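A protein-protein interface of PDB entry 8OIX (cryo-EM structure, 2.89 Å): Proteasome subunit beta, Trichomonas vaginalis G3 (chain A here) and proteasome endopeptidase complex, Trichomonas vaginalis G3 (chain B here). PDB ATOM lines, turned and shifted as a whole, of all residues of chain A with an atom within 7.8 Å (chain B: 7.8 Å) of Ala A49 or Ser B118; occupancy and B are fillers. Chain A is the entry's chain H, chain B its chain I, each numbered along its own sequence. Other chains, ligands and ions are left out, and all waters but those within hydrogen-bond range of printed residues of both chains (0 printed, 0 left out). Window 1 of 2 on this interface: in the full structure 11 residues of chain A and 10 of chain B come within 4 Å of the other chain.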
ATOM      1  N   THR A   1      36.289  17.935   4.770  1.00  0.00           N
ATOM      2  CA  THR A   1      36.483  19.359   5.004  1.00  0.00           C
ATOM      3  C   THR A   1      37.197  19.605   6.325  1.00  0.00           C
ATOM      4  O   THR A   1      36.876  18.992   7.337  1.00  0.00           O
ATOM      5  CB  THR A   1      35.138  20.111   4.983  1.00  0.00           C
ATOM      6  OG1 THR A   1      34.605  20.062   3.657  1.00  0.00           O
ATOM      7  CG2 THR A   1      35.314  21.563   5.390  1.00  0.00           C
ATOM      8  N   THR A  20      36.089  20.437  -2.325  1.00  0.00           N
ATOM      9  CA  THR A  20      34.689  20.045  -2.359  1.00  0.00           C
ATOM     10  C   THR A  20      34.639  18.627  -2.909  1.00  0.00           C
ATOM     11  O   THR A  20      35.235  18.348  -3.952  1.00  0.00           O
ATOM     12  CB  THR A  20      33.867  20.988  -3.237  1.00  0.00           C
ATOM     13  OG1 THR A  20      33.892  22.305  -2.682  1.00  0.00           O
ATOM     14  CG2 THR A  20      32.426  20.517  -3.310  1.00  0.00           C
ATOM     15  N   SER A  21      33.953  17.732  -2.209  1.00  0.00           N
ATOM     16  CA  SER A  21      33.911  16.329  -2.597  1.00  0.00           C
ATOM     17  C   SER A  21      32.480  15.892  -2.864  1.00  0.00           C
ATOM     18  O   SER A  21      31.576  16.183  -2.076  1.00  0.00           O
ATOM     19  CB  SER A  21      34.533  15.439  -1.521  1.00  0.00           C
ATOM     20  OG  SER A  21      35.934  15.629  -1.459  1.00  0.00           O
ATOM     21  N   PRO A  27      34.576  17.782  -7.171  1.00  0.00           N
ATOM     22  CA  PRO A  27      34.084  18.770  -8.146  1.00  0.00           C
ATOM     23  C   PRO A  27      34.872  20.064  -8.134  1.00  0.00           C
ATOM     24  O   PRO A  27      35.174  20.614  -9.199  1.00  0.00           O
ATOM     25  CB  PRO A  27      32.624  18.980  -7.714  1.00  0.00           C
ATOM     26  CG  PRO A  27      32.587  18.518  -6.294  1.00  0.00           C
ATOM     27  CD  PRO A  27      33.487  17.334  -6.294  1.00  0.00           C
ATOM     28  N   THR A  31      38.388  25.301  -3.409  1.00  0.00           N
ATOM     29  CA  THR A  31      37.155  25.804  -2.830  1.00  0.00           C
ATOM     30  C   THR A  31      37.465  26.899  -1.825  1.00  0.00           C
ATOM     31  O   THR A  31      38.411  26.789  -1.041  1.00  0.00           O
ATOM     32  CB  THR A  31      36.374  24.680  -2.147  1.00  0.00           C
ATOM     33  OG1 THR A  31      36.276  23.556  -3.030  1.00  0.00           O
ATOM     34  CG2 THR A  31      34.977  25.153  -1.779  1.00  0.00           C
ATOM     35  N   ARG A  45      33.063  27.065   6.248  1.00  0.00           N
ATOM     36  CA  ARG A  45      31.874  26.277   5.957  1.00  0.00           C
ATOM     37  C   ARG A  45      32.215  24.795   5.860  1.00  0.00           C
ATOM     38  O   ARG A  45      33.158  24.418   5.156  1.00  0.00           O
ATOM     39  CB  ARG A  45      31.246  26.771   4.654  1.00  0.00           C
ATOM     40  CG  ARG A  45      30.694  28.183   4.761  1.00  0.00           C
ATOM     41  CD  ARG A  45      30.053  28.662   3.471  1.00  0.00           C
ATOM     42  NE  ARG A  45      31.023  28.823   2.395  1.00  0.00           N
ATOM     43  CZ  ARG A  45      31.207  27.951   1.414  1.00  0.00           C
ATOM     44  NH1 ARG A  45      30.510  26.830   1.347  1.00  0.00           N
ATOM     45  NH2 ARG A  45      32.115  28.210   0.477  1.00  0.00           N
ATOM     46  N   CYS A  46      31.449  23.956   6.562  1.00  0.00           N
ATOM     47  CA  CYS A  46      31.587  22.510   6.464  1.00  0.00           C
ATOM     48  C   CYS A  46      30.203  21.879   6.421  1.00  0.00           C
ATOM     49  O   CYS A  46      29.216  22.463   6.871  1.00  0.00           O
ATOM     50  CB  CYS A  46      32.387  21.925   7.633  1.00  0.00           C
ATOM     51  SG  CYS A  46      31.651  22.226   9.249  1.00  0.00           S
ATOM     52  N   GLY A  47      30.143  20.660   5.898  1.00  0.00           N
ATOM     53  CA  GLY A  47      28.870  19.995   5.706  1.00  0.00           C
ATOM     54  C   GLY A  47      28.385  20.163   4.284  1.00  0.00           C
ATOM     55  O   GLY A  47      29.200  20.245   3.365  1.00  0.00           O
ATOM     56  N   ASN A  48      27.074  20.228   4.078  1.00  0.00           N
ATOM     57  CA  ASN A  48      26.563  20.396   2.725  1.00  0.00           C
ATOM     58  C   ASN A  48      26.991  21.748   2.172  1.00  0.00           C
ATOM     59  O   ASN A  48      26.802  22.783   2.813  1.00  0.00           O
ATOM     60  CB  ASN A  48      25.041  20.270   2.715  1.00  0.00           C
ATOM     61  CG  ASN A  48      24.448  20.508   1.343  1.00  0.00           C
ATOM     62  OD1 ASN A  48      24.000  21.609   1.033  1.00  0.00           O
ATOM     63  ND2 ASN A  48      24.443  19.473   0.513  1.00  0.00           N
ATOM     64  N   ALA A  49      27.575  21.732   0.971  1.00  0.00           N
ATOM     65  CA  ALA A  49      28.079  22.964   0.373  1.00  0.00           C
ATOM     66  C   ALA A  49      26.949  23.948   0.099  1.00  0.00           C
ATOM     67  O   ALA A  49      27.074  25.146   0.375  1.00  0.00           O
ATOM     68  CB  ALA A  49      28.845  22.647  -0.910  1.00  0.00           C
ATOM     69  N   ALA A  50      25.839  23.457  -0.455  1.00  0.00           N
ATOM     70  CA  ALA A  50      24.708  24.329  -0.742  1.00  0.00           C
ATOM     71  C   ALA A  50      24.140  24.935   0.532  1.00  0.00           C
ATOM     72  O   ALA A  50      23.842  26.135   0.577  1.00  0.00           O
ATOM     73  CB  ALA A  50      23.628  23.556  -1.496  1.00  0.00           C
ATOM     74  N   ASP A  51      23.982  24.121   1.578  1.00  0.00           N
ATOM     75  CA  ASP A  51      23.424  24.628   2.825  1.00  0.00           C
ATOM     76  C   ASP A  51      24.345  25.662   3.454  1.00  0.00           C
ATOM     77  O   ASP A  51      23.880  26.681   3.972  1.00  0.00           O
ATOM     78  CB  ASP A  51      23.162  23.480   3.799  1.00  0.00           C
ATOM     79  CG  ASP A  51      22.160  22.475   3.263  1.00  0.00           C
ATOM     80  OD1 ASP A  51      21.289  22.868   2.464  1.00  0.00           O
ATOM     81  OD2 ASP A  51      22.233  21.292   3.653  1.00  0.00           O
ATOM     82  N   THR A  52      25.657  25.429   3.404  1.00  0.00           N
ATOM     83  CA  THR A  52      26.595  26.377   3.997  1.00  0.00           C
ATOM     84  C   THR A  52      26.672  27.673   3.200  1.00  0.00           C
ATOM     85  O   THR A  52      26.813  28.752   3.781  1.00  0.00           O
ATOM     86  CB  THR A  52      27.978  25.746   4.110  1.00  0.00           C
ATOM     87  OG1 THR A  52      28.405  25.285   2.823  1.00  0.00           O
ATOM     88  CG2 THR A  52      27.956  24.597   5.079  1.00  0.00           C
ATOM     89  N   GLN A  53      26.586  27.595   1.871  1.00  0.00           N
ATOM     90  CA  GLN A  53      26.577  28.820   1.078  1.00  0.00           C
ATOM     91  C   GLN A  53      25.287  29.605   1.278  1.00  0.00           C
ATOM     92  O   GLN A  53      25.311  30.842   1.353  1.00  0.00           O
ATOM     93  CB  GLN A  53      26.805  28.497  -0.394  1.00  0.00           C
ATOM     94  CG  GLN A  53      28.224  28.056  -0.675  1.00  0.00           C
ATOM     95  CD  GLN A  53      28.473  27.776  -2.133  1.00  0.00           C
ATOM     96  OE1 GLN A  53      28.129  26.711  -2.636  1.00  0.00           O
ATOM     97  NE2 GLN A  53      29.073  28.733  -2.827  1.00  0.00           N
ATOM     98  N   PHE A  54      24.150  28.909   1.368  1.00  0.00           N
ATOM     99  CA  PHE A  54      22.918  29.590   1.743  1.00  0.00           C
ATOM    100  C   PHE A  54      23.053  30.233   3.111  1.00  0.00           C
ATOM    101  O   PHE A  54      22.571  31.345   3.329  1.00  0.00           O
ATOM    102  CB  PHE A  54      21.734  28.629   1.745  1.00  0.00           C
ATOM    103  CG  PHE A  54      20.595  29.093   2.613  1.00  0.00           C
ATOM    104  CD1 PHE A  54      19.712  30.056   2.158  1.00  0.00           C
ATOM    105  CD2 PHE A  54      20.412  28.573   3.883  1.00  0.00           C
ATOM    106  CE1 PHE A  54      18.672  30.492   2.950  1.00  0.00           C
ATOM    107  CE2 PHE A  54      19.372  29.009   4.680  1.00  0.00           C
ATOM    108  CZ  PHE A  54      18.500  29.967   4.212  1.00  0.00           C
ATOM    109  N   LEU A  55      23.676  29.528   4.054  1.00  0.00           N
ATOM    110  CA  LEU A  55      23.876  30.081   5.385  1.00  0.00           C
ATOM    111  C   LEU A  55      24.722  31.342   5.326  1.00  0.00           C
ATOM    112  O   LEU A  55      24.408  32.335   5.983  1.00  0.00           O
ATOM    113  CB  LEU A  55      24.528  29.035   6.286  1.00  0.00           C
ATOM    114  CG  LEU A  55      23.922  28.824   7.669  1.00  0.00           C
ATOM    115  CD1 LEU A  55      22.486  28.371   7.560  1.00  0.00           C
ATOM    116  CD2 LEU A  55      24.741  27.797   8.416  1.00  0.00           C
ATOM    117  N   ALA A  56      25.790  31.325   4.530  1.00  0.00           N
ATOM    118  CA  ALA A  56      26.650  32.497   4.416  1.00  0.00           C
ATOM    119  C   ALA A  56      25.896  33.680   3.820  1.00  0.00           C
ATOM    120  O   ALA A  56      25.979  34.805   4.328  1.00  0.00           O
ATOM    121  CB  ALA A  56      27.880  32.159   3.573  1.00  0.00           C
ATOM    122  N   ARG A  57      25.136  33.446   2.746  1.00  0.00           N
ATOM    123  CA  ARG A  57      24.414  34.552   2.122  1.00  0.00           C
ATOM    124  C   ARG A  57      23.283  35.051   3.019  1.00  0.00           C
ATOM    125  O   ARG A  57      23.041  36.261   3.111  1.00  0.00           O
ATOM    126  CB  ARG A  57      23.897  34.142   0.739  1.00  0.00           C
ATOM    127  CG  ARG A  57      22.610  33.336   0.712  1.00  0.00           C
ATOM    128  CD  ARG A  57      22.138  33.107  -0.716  1.00  0.00           C
ATOM    129  NE  ARG A  57      22.725  31.913  -1.311  1.00  0.00           N
ATOM    130  CZ  ARG A  57      22.110  30.743  -1.407  1.00  0.00           C
ATOM    131  NH1 ARG A  57      20.876  30.573  -0.961  1.00  0.00           N
ATOM    132  NH2 ARG A  57      22.749  29.717  -1.961  1.00  0.00           N
ATOM    133  N   SER A  97      22.161  20.596   6.510  1.00  0.00           N
ATOM    134  CA  SER A  97      23.263  19.905   7.177  1.00  0.00           C
ATOM    135  C   SER A  97      24.532  20.748   7.055  1.00  0.00           C
ATOM    136  O   SER A  97      25.476  20.420   6.337  1.00  0.00           O
ATOM    137  CB  SER A  97      23.451  18.512   6.587  1.00  0.00           C
ATOM    138  OG  SER A  97      24.565  17.859   7.171  1.00  0.00           O
ATOM    139  N   ALA A  98      24.534  21.863   7.781  1.00  0.00           N
ATOM    140  CA  ALA A  98      25.588  22.863   7.685  1.00  0.00           C
ATOM    141  C   ALA A  98      26.198  23.124   9.053  1.00  0.00           C
ATOM    142  O   ALA A  98      25.473  23.322  10.033  1.00  0.00           O
ATOM    143  CB  ALA A  98      25.044  24.169   7.101  1.00  0.00           C
ATOM    144  N   THR B  80      25.080  33.785 -11.056  1.00  0.00           N
ATOM    145  CA  THR B  80      25.360  32.599 -10.261  1.00  0.00           C
ATOM    146  C   THR B  80      24.636  32.641  -8.922  1.00  0.00           C
ATOM    147  O   THR B  80      24.137  31.617  -8.454  1.00  0.00           O
ATOM    148  CB  THR B  80      26.864  32.468 -10.054  1.00  0.00           C
ATOM    149  OG1 THR B  80      27.504  32.340 -11.329  1.00  0.00           O
ATOM    150  CG2 THR B  80      27.176  31.253  -9.216  1.00  0.00           C
ATOM    151  N   LEU B  83      20.963  31.914  -9.677  1.00  0.00           N
ATOM    152  CA  LEU B  83      20.810  30.495  -9.986  1.00  0.00           C
ATOM    153  C   LEU B  83      20.939  29.639  -8.735  1.00  0.00           C
ATOM    154  O   LEU B  83      20.157  28.707  -8.524  1.00  0.00           O
ATOM    155  CB  LEU B  83      21.847  30.080 -11.028  1.00  0.00           C
ATOM    156  CG  LEU B  83      21.504  30.398 -12.478  1.00  0.00           C
ATOM    157  CD1 LEU B  83      22.703  30.189 -13.372  1.00  0.00           C
ATOM    158  CD2 LEU B  83      20.372  29.509 -12.912  1.00  0.00           C
ATOM    159  N   ALA B  84      21.935  29.932  -7.898  1.00  0.00           N
ATOM    160  CA  ALA B  84      22.160  29.146  -6.695  1.00  0.00           C
ATOM    161  C   ALA B  84      21.014  29.308  -5.710  1.00  0.00           C
ATOM    162  O   ALA B  84      20.581  28.331  -5.093  1.00  0.00           O
ATOM    163  CB  ALA B  84      23.484  29.544  -6.050  1.00  0.00           C
ATOM    164  N   SER B  85      20.506  30.532  -5.549  1.00  0.00           N
ATOM    165  CA  SER B  85      19.367  30.741  -4.665  1.00  0.00           C
ATOM    166  C   SER B  85      18.135  30.011  -5.178  1.00  0.00           C
ATOM    167  O   SER B  85      17.410  29.382  -4.399  1.00  0.00           O
ATOM    168  CB  SER B  85      19.086  32.235  -4.515  1.00  0.00           C
ATOM    169  OG  SER B  85      18.665  32.798  -5.744  1.00  0.00           O
ATOM    170  N   LEU B  87      18.055  27.324  -7.124  1.00  0.00           N
ATOM    171  CA  LEU B  87      18.248  25.884  -6.998  1.00  0.00           C
ATOM    172  C   LEU B  87      18.211  25.434  -5.546  1.00  0.00           C
ATOM    173  O   LEU B  87      17.811  24.301  -5.261  1.00  0.00           O
ATOM    174  CB  LEU B  87      19.566  25.471  -7.650  1.00  0.00           C
ATOM    175  CG  LEU B  87      19.583  25.520  -9.176  1.00  0.00           C
ATOM    176  CD1 LEU B  87      20.977  25.316  -9.713  1.00  0.00           C
ATOM    177  CD2 LEU B  87      18.662  24.457  -9.718  1.00  0.00           C
ATOM    178  N   PHE B  88      18.630  26.296  -4.618  1.00  0.00           N
ATOM    179  CA  PHE B  88      18.545  25.958  -3.205  1.00  0.00           C
ATOM    180  C   PHE B  88      17.103  25.986  -2.719  1.00  0.00           C
ATOM    181  O   PHE B  88      16.688  25.120  -1.939  1.00  0.00           O
ATOM    182  CB  PHE B  88      19.404  26.917  -2.384  1.00  0.00           C
ATOM    183  CG  PHE B  88      19.476  26.561  -0.932  1.00  0.00           C
ATOM    184  CD1 PHE B  88      20.389  25.627  -0.484  1.00  0.00           C
ATOM    185  CD2 PHE B  88      18.621  27.149  -0.017  1.00  0.00           C
ATOM    186  CE1 PHE B  88      20.456  25.293   0.848  1.00  0.00           C
ATOM    187  CE2 PHE B  88      18.680  26.813   1.316  1.00  0.00           C
ATOM    188  CZ  PHE B  88      19.601  25.885   1.749  1.00  0.00           C
ATOM    189  N   LEU B  98      24.624  23.488 -13.414  1.00  0.00           N
ATOM    190  CA  LEU B  98      24.911  24.523 -14.390  1.00  0.00           C
ATOM    191  C   LEU B  98      26.359  24.975 -14.286  1.00  0.00           C
ATOM    192  O   LEU B  98      26.983  24.885 -13.226  1.00  0.00           O
ATOM    193  CB  LEU B  98      23.976  25.714 -14.185  1.00  0.00           C
ATOM    194  CG  LEU B  98      22.505  25.307 -14.196  1.00  0.00           C
ATOM    195  CD1 LEU B  98      21.651  26.389 -13.609  1.00  0.00           C
ATOM    196  CD2 LEU B  98      22.060  25.002 -15.610  1.00  0.00           C
ATOM    197  N   TYR B 111      31.545  29.996 -13.061  1.00  0.00           N
ATOM    198  CA  TYR B 111      30.987  29.477 -11.823  1.00  0.00           C
ATOM    199  C   TYR B 111      30.301  28.146 -12.086  1.00  0.00           C
ATOM    200  O   TYR B 111      29.696  27.949 -13.140  1.00  0.00           O
ATOM    201  CB  TYR B 111      29.972  30.449 -11.225  1.00  0.00           C
ATOM    202  CG  TYR B 111      30.558  31.703 -10.623  1.00  0.00           C
ATOM    203  CD1 TYR B 111      30.979  32.749 -11.428  1.00  0.00           C
ATOM    204  CD2 TYR B 111      30.668  31.849  -9.248  1.00  0.00           C
ATOM    205  CE1 TYR B 111      31.504  33.900 -10.883  1.00  0.00           C
ATOM    206  CE2 TYR B 111      31.191  32.997  -8.694  1.00  0.00           C
ATOM    207  CZ  TYR B 111      31.609  34.019  -9.517  1.00  0.00           C
ATOM    208  OH  TYR B 111      32.135  35.165  -8.970  1.00  0.00           O
ATOM    209  N   GLN B 112      30.409  27.229 -11.138  1.00  0.00           N
ATOM    210  CA  GLN B 112      29.572  26.041 -11.118  1.00  0.00           C
ATOM    211  C   GLN B 112      28.424  26.282 -10.152  1.00  0.00           C
ATOM    212  O   GLN B 112      28.584  26.964  -9.139  1.00  0.00           O
ATOM    213  CB  GLN B 112      30.379  24.805 -10.702  1.00  0.00           C
ATOM    214  CG  GLN B 112      29.598  23.674 -10.052  1.00  0.00           C
ATOM    215  CD  GLN B 112      29.493  23.816  -8.546  1.00  0.00           C
ATOM    216  OE1 GLN B 112      30.204  24.611  -7.936  1.00  0.00           O
ATOM    217  NE2 GLN B 112      28.605  23.039  -7.941  1.00  0.00           N
ATOM    218  N   VAL B 113      27.260  25.730 -10.478  1.00  0.00           N
ATOM    219  CA  VAL B 113      26.101  25.759  -9.595  1.00  0.00           C
ATOM    220  C   VAL B 113      25.533  24.349  -9.571  1.00  0.00           C
ATOM    221  O   VAL B 113      25.009  23.869 -10.582  1.00  0.00           O
ATOM    222  CB  VAL B 113      25.038  26.769 -10.049  1.00  0.00           C
ATOM    223  CG1 VAL B 113      23.994  26.944  -8.971  1.00  0.00           C
ATOM    224  CG2 VAL B 113      25.669  28.107 -10.396  1.00  0.00           C
ATOM    225  N   ALA B 114      25.632  23.685  -8.425  1.00  0.00           N
ATOM    226  CA  ALA B 114      25.093  22.346  -8.294  1.00  0.00           C
ATOM    227  C   ALA B 114      23.570  22.401  -8.250  1.00  0.00           C
ATOM    228  O   ALA B 114      22.988  23.442  -7.937  1.00  0.00           O
ATOM    229  CB  ALA B 114      25.638  21.674  -7.037  1.00  0.00           C
ATOM    230  N   PRO B 115      22.898  21.292  -8.573  1.00  0.00           N
ATOM    231  CA  PRO B 115      21.426  21.297  -8.535  1.00  0.00           C
ATOM    232  C   PRO B 115      20.859  21.708  -7.189  1.00  0.00           C
ATOM    233  O   PRO B 115      19.741  22.233  -7.133  1.00  0.00           O
ATOM    234  CB  PRO B 115      21.063  19.849  -8.883  1.00  0.00           C
ATOM    235  CG  PRO B 115      22.212  19.363  -9.683  1.00  0.00           C
ATOM    236  CD  PRO B 115      23.426  20.023  -9.107  1.00  0.00           C
ATOM    237  N   HIS B 116      21.595  21.491  -6.103  1.00  0.00           N
ATOM    238  CA  HIS B 116      21.126  21.830  -4.770  1.00  0.00           C
ATOM    239  C   HIS B 116      21.409  23.277  -4.391  1.00  0.00           C
ATOM    240  O   HIS B 116      21.041  23.694  -3.290  1.00  0.00           O
ATOM    241  CB  HIS B 116      21.761  20.899  -3.734  1.00  0.00           C
ATOM    242  CG  HIS B 116      21.211  19.508  -3.759  1.00  0.00           C
ATOM    243  ND1 HIS B 116      21.698  18.532  -4.601  1.00  0.00           N
ATOM    244  CD2 HIS B 116      20.215  18.930  -3.048  1.00  0.00           C
ATOM    245  CE1 HIS B 116      21.026  17.411  -4.407  1.00  0.00           C
ATOM    246  NE2 HIS B 116      20.120  17.626  -3.469  1.00  0.00           N
ATOM    247  N   GLY B 117      22.035  24.052  -5.274  1.00  0.00           N
ATOM    248  CA  GLY B 117      22.299  25.449  -5.007  1.00  0.00           C
ATOM    249  C   GLY B 117      23.703  25.776  -4.555  1.00  0.00           C
ATOM    250  O   GLY B 117      23.965  26.932  -4.206  1.00  0.00           O
ATOM    251  N   SER B 118      24.612  24.806  -4.540  1.00  0.00           N
ATOM    252  CA  SER B 118      25.998  25.054  -4.156  1.00  0.00           C
ATOM    253  C   SER B 118      26.761  25.565  -5.370  1.00  0.00           C
ATOM    254  O   SER B 118      26.946  24.836  -6.349  1.00  0.00           O
ATOM    255  CB  SER B 118      26.651  23.790  -3.607  1.00  0.00           C
ATOM    256  OG  SER B 118      27.148  22.972  -4.649  1.00  0.00           O
ATOM    257  N   PHE B 119      27.203  26.815  -5.309  1.00  0.00           N
ATOM    258  CA  PHE B 119      27.978  27.408  -6.384  1.00  0.00           C
ATOM    259  C   PHE B 119      29.439  27.529  -5.972  1.00  0.00           C
ATOM    260  O   PHE B 119      29.804  27.368  -4.804  1.00  0.00           O
ATOM    261  CB  PHE B 119      27.407  28.777  -6.777  1.00  0.00           C
ATOM    262  CG  PHE B 119      27.610  29.849  -5.745  1.00  0.00           C
ATOM    263  CD1 PHE B 119      28.741  30.649  -5.770  1.00  0.00           C
ATOM    264  CD2 PHE B 119      26.670  30.062  -4.752  1.00  0.00           C
ATOM    265  CE1 PHE B 119      28.931  31.636  -4.826  1.00  0.00           C
ATOM    266  CE2 PHE B 119      26.854  31.048  -3.805  1.00  0.00           C
ATOM    267  CZ  PHE B 119      27.986  31.836  -3.842  1.00  0.00           C
ATOM    268  N   SER B 120      30.275  27.816  -6.963  1.00  0.00           N
ATOM    269  CA  SER B 120      31.712  27.942  -6.748  1.00  0.00           C
ATOM    270  C   SER B 120      32.389  28.578  -7.952  1.00  0.00           C
ATOM    271  O   SER B 120      32.201  28.123  -9.081  1.00  0.00           O
ATOM    272  CB  SER B 120      32.334  26.574  -6.466  1.00  0.00           C
ATOM    273  OG  SER B 120      32.317  25.763  -7.626  1.00  0.00           O
ATOM    274  N   GLN B 122      35.368  28.824 -10.233  1.00  0.00           N
ATOM    275  CA  GLN B 122      36.501  27.987 -10.590  1.00  0.00           C
ATOM    276  C   GLN B 122      37.012  28.405 -11.957  1.00  0.00           C
ATOM    277  O   GLN B 122      36.226  28.829 -12.813  1.00  0.00           O
ATOM    278  CB  GLN B 122      36.135  26.497 -10.620  1.00  0.00           C
ATOM    279  CG  GLN B 122      35.483  25.969  -9.366  1.00  0.00           C
ATOM    280  CD  GLN B 122      35.290  24.474  -9.418  1.00  0.00           C
ATOM    281  OE1 GLN B 122      36.250  23.720  -9.563  1.00  0.00           O
ATOM    282  NE2 GLN B 122      34.043  24.033  -9.311  1.00  0.00           N
ATOM    283  N   GLN B 127      30.880  19.465 -15.748  1.00  0.00           N
ATOM    284  CA  GLN B 127      29.709  18.882 -15.116  1.00  0.00           C
ATOM    285  C   GLN B 127      29.010  17.968 -16.113  1.00  0.00           C
ATOM    286  O   GLN B 127      29.289  17.991 -17.316  1.00  0.00           O
ATOM    287  CB  GLN B 127      28.751  19.955 -14.588  1.00  0.00           C
ATOM    288  CG  GLN B 127      29.400  20.900 -13.593  1.00  0.00           C
ATOM    289  CD  GLN B 127      28.477  21.279 -12.460  1.00  0.00           C
ATOM    290  OE1 GLN B 127      28.702  20.903 -11.311  1.00  0.00           O
ATOM    291  NE2 GLN B 127      27.437  22.038 -12.772  1.00  0.00           N
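Among the printed residues, merely in contact across the chains: Asp A51 with Phe B88, Gln A53 with Ser B118, Ala A50 with His B116, Phe A54 with Phe B88, Ala A50 with Ser B118, Ala A50 with Phe B88, Ala A49 with Ser B118, Arg A57 with Gly B117 and Ala A50 with Gly B117.
The side-chain amide oxygen (OD1) of Asn A48 lies within hydrogen-bond range of the backbone NH (N) of Ala A50 (3.0 Å).
N of Asp A51 is in hydrogen-bond range of OD1 of Asn A48, 2.6 Å away.
The backbone carbonyl oxygen (O) of Ala A49 sits at hydrogen-bond distance from the side-chain hydroxyl (OG1) of Thr A52 (2.8 Å).
The side-chain carboxylate (OD2) of Asp A51 lies within hydrogen-bond range of the backbone NH (N) of Ser A97, 2.9 Å away.
The side-chain amide nitrogen (NE2) of Gln B112 lies within hydrogen-bond range of the backbone carbonyl oxygen (O) of Ser B118.
OG of Ser B120 lies within hydrogen-bond range of NE2 of Gln B122 (3.0 Å).
Hydrophobic or aromatic side chains of chain A within 4 Å of the printed part of chain B: Ala A49, Ala A50 and Phe A54.
Along chain A the printed residues that touch a printed residue of chain B span positions 27 to 57.
Hydrophobic or aromatic side chains of chain B within 4 Å of the printed part of chain A: Phe B88, His B116 and Phe B119.
Among the printed residues, no Asp or Glu carboxylate lies within 4 Å of a Lys or Arg side-chain nitrogen of the other chain.
Of the printed residues of chain B, Pro A27 touches Gln B122.
Ala A49 touches just one residue of chain B: Ser B118 (3.7 Å).
Ala A50 touches just these residues of chain B: Phe B88, His B116, Gly B117 and Ser B118.
Printed residues of chain B within 4 Å of Gln A53: Ser B118 and Phe B119.
Ala B114 touches none of the printed residues of chain A.
Gly B117 touches just these residues of chain A: Ala A50 (3.8 Å) and Arg A57 (3.8 Å).
Ser B118 touches three residues of chain A.
Printed residues of chain A within 4 Å of Gln B122: Pro A27.
The nearest residue of chain B that does not touch Ala A49 is Gly B117 (5.8 Å).
O of Pro A27 sits close to OE1 of Gln B122 (3.3 Å).
NE2 of Gln A53 is in hydrogen-bond range of O of Phe B119 (2.5 Å).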
